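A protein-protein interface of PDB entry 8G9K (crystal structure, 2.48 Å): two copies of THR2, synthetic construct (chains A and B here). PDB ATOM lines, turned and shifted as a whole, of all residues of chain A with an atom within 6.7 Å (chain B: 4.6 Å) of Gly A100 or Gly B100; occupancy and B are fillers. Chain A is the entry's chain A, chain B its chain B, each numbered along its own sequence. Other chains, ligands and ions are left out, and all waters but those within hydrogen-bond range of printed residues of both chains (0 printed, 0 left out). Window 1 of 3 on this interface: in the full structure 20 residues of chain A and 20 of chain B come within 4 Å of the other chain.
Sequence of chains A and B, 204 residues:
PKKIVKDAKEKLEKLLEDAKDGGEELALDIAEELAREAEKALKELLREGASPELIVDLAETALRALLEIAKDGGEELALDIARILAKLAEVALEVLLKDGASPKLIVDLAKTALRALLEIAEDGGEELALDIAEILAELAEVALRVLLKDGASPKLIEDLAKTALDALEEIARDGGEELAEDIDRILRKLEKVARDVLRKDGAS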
ATOM      1  N   LEU A  46     -18.120   4.177   5.136  1.00  0.00           N
ATOM      2  CA  LEU A  46     -18.543   3.329   6.246  1.00  0.00           C
ATOM      3  C   LEU A  46     -18.222   1.863   5.979  1.00  0.00           C
ATOM      4  O   LEU A  46     -17.797   1.139   6.887  1.00  0.00           O
ATOM      5  CB  LEU A  46     -20.040   3.510   6.498  1.00  0.00           C
ATOM      6  CG  LEU A  46     -20.662   2.609   7.565  1.00  0.00           C
ATOM      7  CD1 LEU A  46     -20.083   2.925   8.935  1.00  0.00           C
ATOM      8  CD2 LEU A  46     -22.177   2.742   7.572  1.00  0.00           C
ATOM      9  N   PRO A  52     -13.834   8.593  11.456  1.00  0.00           N
ATOM     10  CA  PRO A  52     -14.919   9.582  11.539  1.00  0.00           C
ATOM     11  C   PRO A  52     -14.521  10.956  11.033  1.00  0.00           C
ATOM     12  O   PRO A  52     -15.381  11.698  10.541  1.00  0.00           O
ATOM     13  CB  PRO A  52     -15.252   9.610  13.037  1.00  0.00           C
ATOM     14  CG  PRO A  52     -14.771   8.302  13.560  1.00  0.00           C
ATOM     15  CD  PRO A  52     -13.550   7.970  12.760  1.00  0.00           C
ATOM     16  N   GLU A  53     -13.242  11.319  11.139  1.00  0.00           N
ATOM     17  CA  GLU A  53     -12.804  12.629  10.669  1.00  0.00           C
ATOM     18  C   GLU A  53     -12.886  12.725   9.149  1.00  0.00           C
ATOM     19  O   GLU A  53     -13.226  13.784   8.608  1.00  0.00           O
ATOM     20  CB  GLU A  53     -11.382  12.909  11.159  1.00  0.00           C
ATOM     21  CG  GLU A  53     -10.847  14.286  10.799  1.00  0.00           C
ATOM     22  CD  GLU A  53      -9.591  14.640  11.574  1.00  0.00           C
ATOM     23  OE1 GLU A  53      -9.507  14.279  12.767  1.00  0.00           O
ATOM     24  OE2 GLU A  53      -8.684  15.270  10.990  1.00  0.00           O
ATOM     25  N   VAL A  95     -24.329   8.031   9.526  1.00  0.00           N
ATOM     26  CA  VAL A  95     -23.113   7.307   9.162  1.00  0.00           C
ATOM     27  C   VAL A  95     -22.059   7.454  10.253  1.00  0.00           C
ATOM     28  O   VAL A  95     -21.364   6.490  10.601  1.00  0.00           O
ATOM     29  CB  VAL A  95     -22.592   7.789   7.794  1.00  0.00           C
ATOM     30  CG1 VAL A  95     -21.170   7.312   7.557  1.00  0.00           C
ATOM     31  CG2 VAL A  95     -23.503   7.297   6.683  1.00  0.00           C
ATOM     32  N   LEU A  96     -21.927   8.659  10.815  1.00  0.00           N
ATOM     33  CA  LEU A  96     -20.992   8.863  11.917  1.00  0.00           C
ATOM     34  C   LEU A  96     -21.352   7.992  13.114  1.00  0.00           C
ATOM     35  O   LEU A  96     -20.470   7.410  13.757  1.00  0.00           O
ATOM     36  CB  LEU A  96     -20.965  10.337  12.321  1.00  0.00           C
ATOM     37  CG  LEU A  96     -20.213  11.313  11.417  1.00  0.00           C
ATOM     38  CD1 LEU A  96     -20.337  12.726  11.957  1.00  0.00           C
ATOM     39  CD2 LEU A  96     -18.751  10.914  11.301  1.00  0.00           C
ATOM     40  N   LEU A  97     -22.647   7.888  13.426  1.00  0.00           N
ATOM     41  CA  LEU A  97     -23.078   7.045  14.536  1.00  0.00           C
ATOM     42  C   LEU A  97     -22.785   5.576  14.261  1.00  0.00           C
ATOM     43  O   LEU A  97     -22.369   4.840  15.164  1.00  0.00           O
ATOM     44  CB  LEU A  97     -24.570   7.252  14.799  1.00  0.00           C
ATOM     45  CG  LEU A  97     -25.198   6.393  15.898  1.00  0.00           C
ATOM     46  CD1 LEU A  97     -24.619   6.754  17.257  1.00  0.00           C
ATOM     47  CD2 LEU A  97     -26.711   6.542  15.897  1.00  0.00           C
ATOM     48  N   LYS A  98     -22.995   5.129  13.020  1.00  0.00           N
ATOM     49  CA  LYS A  98     -22.711   3.739  12.678  1.00  0.00           C
ATOM     50  C   LYS A  98     -21.213   3.469  12.606  1.00  0.00           C
ATOM     51  O   LYS A  98     -20.774   2.344  12.870  1.00  0.00           O
ATOM     52  CB  LYS A  98     -23.379   3.378  11.351  1.00  0.00           C
ATOM     53  CG  LYS A  98     -24.898   3.425  11.383  1.00  0.00           C
ATOM     54  CD  LYS A  98     -25.486   3.012  10.043  1.00  0.00           C
ATOM     55  CE  LYS A  98     -27.003   2.932  10.101  1.00  0.00           C
ATOM     56  NZ  LYS A  98     -27.582   2.469   8.810  1.00  0.00           N
ATOM     57  N   ASP A  99     -20.416   4.480  12.254  1.00  0.00           N
ATOM     58  CA  ASP A  99     -18.972   4.308  12.157  1.00  0.00           C
ATOM     59  C   ASP A  99     -18.291   4.268  13.519  1.00  0.00           C
ATOM     60  O   ASP A  99     -17.157   3.787  13.618  1.00  0.00           O
ATOM     61  CB  ASP A  99     -18.370   5.432  11.307  1.00  0.00           C
ATOM     62  CG  ASP A  99     -16.892   5.235  11.035  1.00  0.00           C
ATOM     63  OD1 ASP A  99     -16.524   4.160  10.519  1.00  0.00           O
ATOM     64  OD2 ASP A  99     -16.099   6.153  11.333  1.00  0.00           O
ATOM     65  N   GLY A 100     -18.958   4.743  14.566  1.00  0.00           N
ATOM     66  CA  GLY A 100     -18.339   4.829  15.871  1.00  0.00           C
ATOM     67  C   GLY A 100     -17.683   6.157  16.160  1.00  0.00           C
ATOM     68  O   GLY A 100     -16.661   6.195  16.853  1.00  0.00           O
ATOM     69  N   ALA A 101     -18.238   7.251  15.645  1.00  0.00           N
ATOM     70  CA  ALA A 101     -17.649   8.566  15.838  1.00  0.00           C
ATOM     71  C   ALA A 101     -17.824   9.035  17.279  1.00  0.00           C
ATOM     72  O   ALA A 101     -18.681   8.551  18.023  1.00  0.00           O
ATOM     73  CB  ALA A 101     -18.278   9.579  14.882  1.00  0.00           C
ATOM     74  N   SER A 102     -16.992   9.995  17.667  1.00  0.00           N
ATOM     75  CA  SER A 102     -17.102  10.613  18.976  1.00  0.00           C
ATOM     76  C   SER A 102     -18.251  11.614  18.987  1.00  0.00           C
ATOM     77  O   SER A 102     -18.688  12.084  17.933  1.00  0.00           O
ATOM     78  CB  SER A 102     -15.795  11.311  19.340  1.00  0.00           C
ATOM     79  OG  SER A 102     -15.564  12.428  18.498  1.00  0.00           O
ATOM     80  N   PRO A 103     -18.771  11.954  20.169  1.00  0.00           N
ATOM     81  CA  PRO A 103     -19.829  12.975  20.221  1.00  0.00           C
ATOM     82  C   PRO A 103     -19.371  14.337  19.732  1.00  0.00           C
ATOM     83  O   PRO A 103     -20.183  15.092  19.182  1.00  0.00           O
ATOM     84  CB  PRO A 103     -20.214  13.006  21.706  1.00  0.00           C
ATOM     85  CG  PRO A 103     -19.785  11.679  22.241  1.00  0.00           C
ATOM     86  CD  PRO A 103     -18.543  11.329  21.483  1.00  0.00           C
ATOM     87  N   LEU A 105     -17.299  15.080  17.225  1.00  0.00           N
ATOM     88  CA  LEU A 105     -17.356  15.146  15.768  1.00  0.00           C
ATOM     89  C   LEU A 105     -18.796  15.231  15.275  1.00  0.00           C
ATOM     90  O   LEU A 105     -19.085  15.918  14.286  1.00  0.00           O
ATOM     91  CB  LEU A 105     -16.646  13.936  15.162  1.00  0.00           C
ATOM     92  CG  LEU A 105     -15.128  13.946  15.335  1.00  0.00           C
ATOM     93  CD1 LEU A 105     -14.513  12.665  14.797  1.00  0.00           C
ATOM     94  CD2 LEU A 105     -14.534  15.161  14.642  1.00  0.00           C
ATOM     95  N   ASP A 150     -25.144   8.019  20.870  1.00  0.00           N
ATOM     96  CA  ASP A 150     -23.697   7.867  20.804  1.00  0.00           C
ATOM     97  C   ASP A 150     -23.023   7.970  22.168  1.00  0.00           C
ATOM     98  O   ASP A 150     -21.793   7.876  22.246  1.00  0.00           O
ATOM     99  CB  ASP A 150     -23.113   8.916  19.848  1.00  0.00           C
ATOM    100  CG  ASP A 150     -21.686   8.606  19.436  1.00  0.00           C
ATOM    101  OD1 ASP A 150     -21.414   7.446  19.064  1.00  0.00           O
ATOM    102  OD2 ASP A 150     -20.841   9.524  19.480  1.00  0.00           O
ATOM    103  N   PRO B  52     -12.475   3.400  13.997  1.00  0.00           N
ATOM    104  CA  PRO B  52     -12.152   3.002  15.375  1.00  0.00           C
ATOM    105  C   PRO B  52     -12.385   1.527  15.641  1.00  0.00           C
ATOM    106  O   PRO B  52     -11.726   0.953  16.517  1.00  0.00           O
ATOM    107  CB  PRO B  52     -13.083   3.883  16.221  1.00  0.00           C
ATOM    108  CG  PRO B  52     -13.433   5.035  15.338  1.00  0.00           C
ATOM    109  CD  PRO B  52     -13.480   4.476  13.951  1.00  0.00           C
ATOM    110  N   LEU B  96      -7.381   5.770  19.831  1.00  0.00           N
ATOM    111  CA  LEU B  96      -8.825   5.863  19.635  1.00  0.00           C
ATOM    112  C   LEU B  96      -9.327   7.279  19.884  1.00  0.00           C
ATOM    113  O   LEU B  96     -10.217   7.765  19.175  1.00  0.00           O
ATOM    114  CB  LEU B  96      -9.547   4.873  20.550  1.00  0.00           C
ATOM    115  CG  LEU B  96      -9.544   3.400  20.139  1.00  0.00           C
ATOM    116  CD1 LEU B  96     -10.208   2.559  21.213  1.00  0.00           C
ATOM    117  CD2 LEU B  96     -10.249   3.219  18.802  1.00  0.00           C
ATOM    118  N   LEU B  97      -8.767   7.960  20.886  1.00  0.00           N
ATOM    119  CA  LEU B  97      -9.171   9.334  21.162  1.00  0.00           C
ATOM    120  C   LEU B  97      -8.784  10.261  20.016  1.00  0.00           C
ATOM    121  O   LEU B  97      -9.549  11.162  19.652  1.00  0.00           O
ATOM    122  CB  LEU B  97      -8.546   9.809  22.472  1.00  0.00           C
ATOM    123  CG  LEU B  97      -8.911  11.225  22.918  1.00  0.00           C
ATOM    124  CD1 LEU B  97     -10.388  11.312  23.268  1.00  0.00           C
ATOM    125  CD2 LEU B  97      -8.048  11.662  24.092  1.00  0.00           C
ATOM    126  N   LYS B  98      -7.600  10.054  19.436  1.00  0.00           N
ATOM    127  CA  LYS B  98      -7.171  10.869  18.306  1.00  0.00           C
ATOM    128  C   LYS B  98      -7.926  10.517  17.033  1.00  0.00           C
ATOM    129  O   LYS B  98      -8.174  11.396  16.200  1.00  0.00           O
ATOM    130  CB  LYS B  98      -5.665  10.711  18.087  1.00  0.00           C
ATOM    131  CG  LYS B  98      -4.815  11.211  19.241  1.00  0.00           C
ATOM    132  CD  LYS B  98      -3.342  10.921  19.009  1.00  0.00           C
ATOM    133  CE  LYS B  98      -2.500  11.395  20.180  1.00  0.00           C
ATOM    134  NZ  LYS B  98      -1.070  11.012  20.024  1.00  0.00           N
ATOM    135  N   ASP B  99      -8.296   9.246  16.862  1.00  0.00           N
ATOM    136  CA  ASP B  99      -9.073   8.834  15.699  1.00  0.00           C
ATOM    137  C   ASP B  99     -10.520   9.302  15.771  1.00  0.00           C
ATOM    138  O   ASP B  99     -11.226   9.239  14.757  1.00  0.00           O
ATOM    139  CB  ASP B  99      -9.016   7.310  15.555  1.00  0.00           C
ATOM    140  CG  ASP B  99      -9.622   6.821  14.253  1.00  0.00           C
ATOM    141  OD1 ASP B  99      -9.182   7.283  13.179  1.00  0.00           O
ATOM    142  OD2 ASP B  99     -10.531   5.966  14.302  1.00  0.00           O
ATOM    143  N   GLY B 100     -10.971   9.780  16.928  1.00  0.00           N
ATOM    144  CA  GLY B 100     -12.348  10.196  17.089  1.00  0.00           C
ATOM    145  C   GLY B 100     -13.299   9.083  17.454  1.00  0.00           C
ATOM    146  O   GLY B 100     -14.456   9.102  17.017  1.00  0.00           O
ATOM    147  N   ALA B 101     -12.853   8.115  18.251  1.00  0.00           N
ATOM    148  CA  ALA B 101     -13.666   6.951  18.558  1.00  0.00           C
ATOM    149  C   ALA B 101     -14.840   7.320  19.461  1.00  0.00           C
ATOM    150  O   ALA B 101     -14.837   8.343  20.152  1.00  0.00           O
ATOM    151  CB  ALA B 101     -12.819   5.867  19.225  1.00  0.00           C
ATOM    152  N   SER B 102     -15.854   6.464  19.443  1.00  0.00           N
ATOM    153  CA  SER B 102     -17.024   6.638  20.282  1.00  0.00           C
ATOM    154  C   SER B 102     -16.712   6.225  21.716  1.00  0.00           C
ATOM    155  O   SER B 102     -15.764   5.477  21.965  1.00  0.00           O
ATOM    156  CB  SER B 102     -18.185   5.813  19.736  1.00  0.00           C
ATOM    157  OG  SER B 102     -17.872   4.432  19.741  1.00  0.00           O
ATOM    158  N   LEU B 105     -16.734   2.236  22.113  1.00  0.00           N
ATOM    159  CA  LEU B 105     -15.560   1.491  21.667  1.00  0.00           C
ATOM    160  C   LEU B 105     -14.391   1.667  22.629  1.00  0.00           C
ATOM    161  O   LEU B 105     -13.612   0.731  22.846  1.00  0.00           O
ATOM    162  CB  LEU B 105     -15.172   1.924  20.255  1.00  0.00           C
ATOM    163  CG  LEU B 105     -16.146   1.492  19.158  1.00  0.00           C
ATOM    164  CD1 LEU B 105     -15.787   2.135  17.830  1.00  0.00           C
ATOM    165  CD2 LEU B 105     -16.159  -0.026  19.033  1.00  0.00           C
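The backbone carbonyl oxygen (O) of Gly A100 sits at hydrogen-bond distance from the backbone NH (N) of Ser B102, 2.7 Å away. The backbone NH (N) of Ser A102 lies within hydrogen-bond range of the backbone carbonyl oxygen (O) of Gly B100.
The backbone carbonyl oxygen (O) of Leu A96 lies within hydrogen-bond range of the backbone NH (N) of Ala A101 (2.9 Å). The backbone NH (N) of Ala B101 is in hydrogen-bond range of the backbone carbonyl oxygen (O) of Leu B96. The side-chain hydroxyl of Ser A102 lies within hydrogen-bond range of the backbone NH of Leu A105. The side-chain hydroxyl (OG) of Ser B102 sits at hydrogen-bond distance from the backbone NH (N) of Leu B105, 3.4 Å away.
Pro A52 touches Pro B52 (CD to CD, 3.7 Å). Pro A52 touches Asp B99. O of Gly B100 touches CG of Pro A52 (3.6 Å). O of Asp A99 touches CD of Pro B52, at 3.8 Å. Pro B52 touches Gly A100 (CG to O, 3.7 Å). Gly A100 touches Gly B100 (O to O, 3.7 Å). Ala B101 touches Gly A100 (C to O, 3.4 Å). Ala A101 touches Gly B100 (C to O, 3.4 Å). Ala A101 touches Ser B102. Ser A102 touches Ala B101.
Gly A100 touches just these residues of chain B: Pro B52, Gly B100, Ala B101 and Ser B102. Printed residues of chain A within 4 Å of Gly B100: Pro A52 (3.6 Å), Gly A100 (3.7 Å), Ala A101 (3.4 Å) and Ser A102 (2.8 Å). Of the printed residues of chain A, Pro B52 touches Pro A52 (3.7 Å), Asp A99 (3.8 Å) and Gly A100 (3.7 Å). Printed residues of chain A within 4 Å of Asp B99: Pro A52. Printed residues of chain B within 4 Å of Asp A150: Ser B102. Glu A53 touches none of the printed residues of chain B. The nearest printed residue of chain A that does not touch Gly B100 is Leu A105 (4.005 Å). The nearest printed residue of chain B that does not touch Pro A52 is Ala B101 (5.1 Å).
Hydrophobic or aromatic side chains of chain A within 4 Å of the printed part of chain B: Pro A52. Of the 9 printed residues of chain B, 5 touch a printed residue of chain A. Among the printed residues, 13 pairs touch across the chains. Among the printed residues, no Asp or Glu carboxylate lies within 4 Å of a Lys or Arg side-chain nitrogen of the other chain.
Pro B52 touches its own counterpart, Pro A52. Pro A52 touches Asp B99, and with the chains exchanged Asp A99 touches Pro B52. Gly A100 touches Ala B101, and with the chains exchanged Ala A101 touches Gly B100. Ala A101 touches Ser B102, and with the chains exchanged Ser A102 touches Ala B101.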
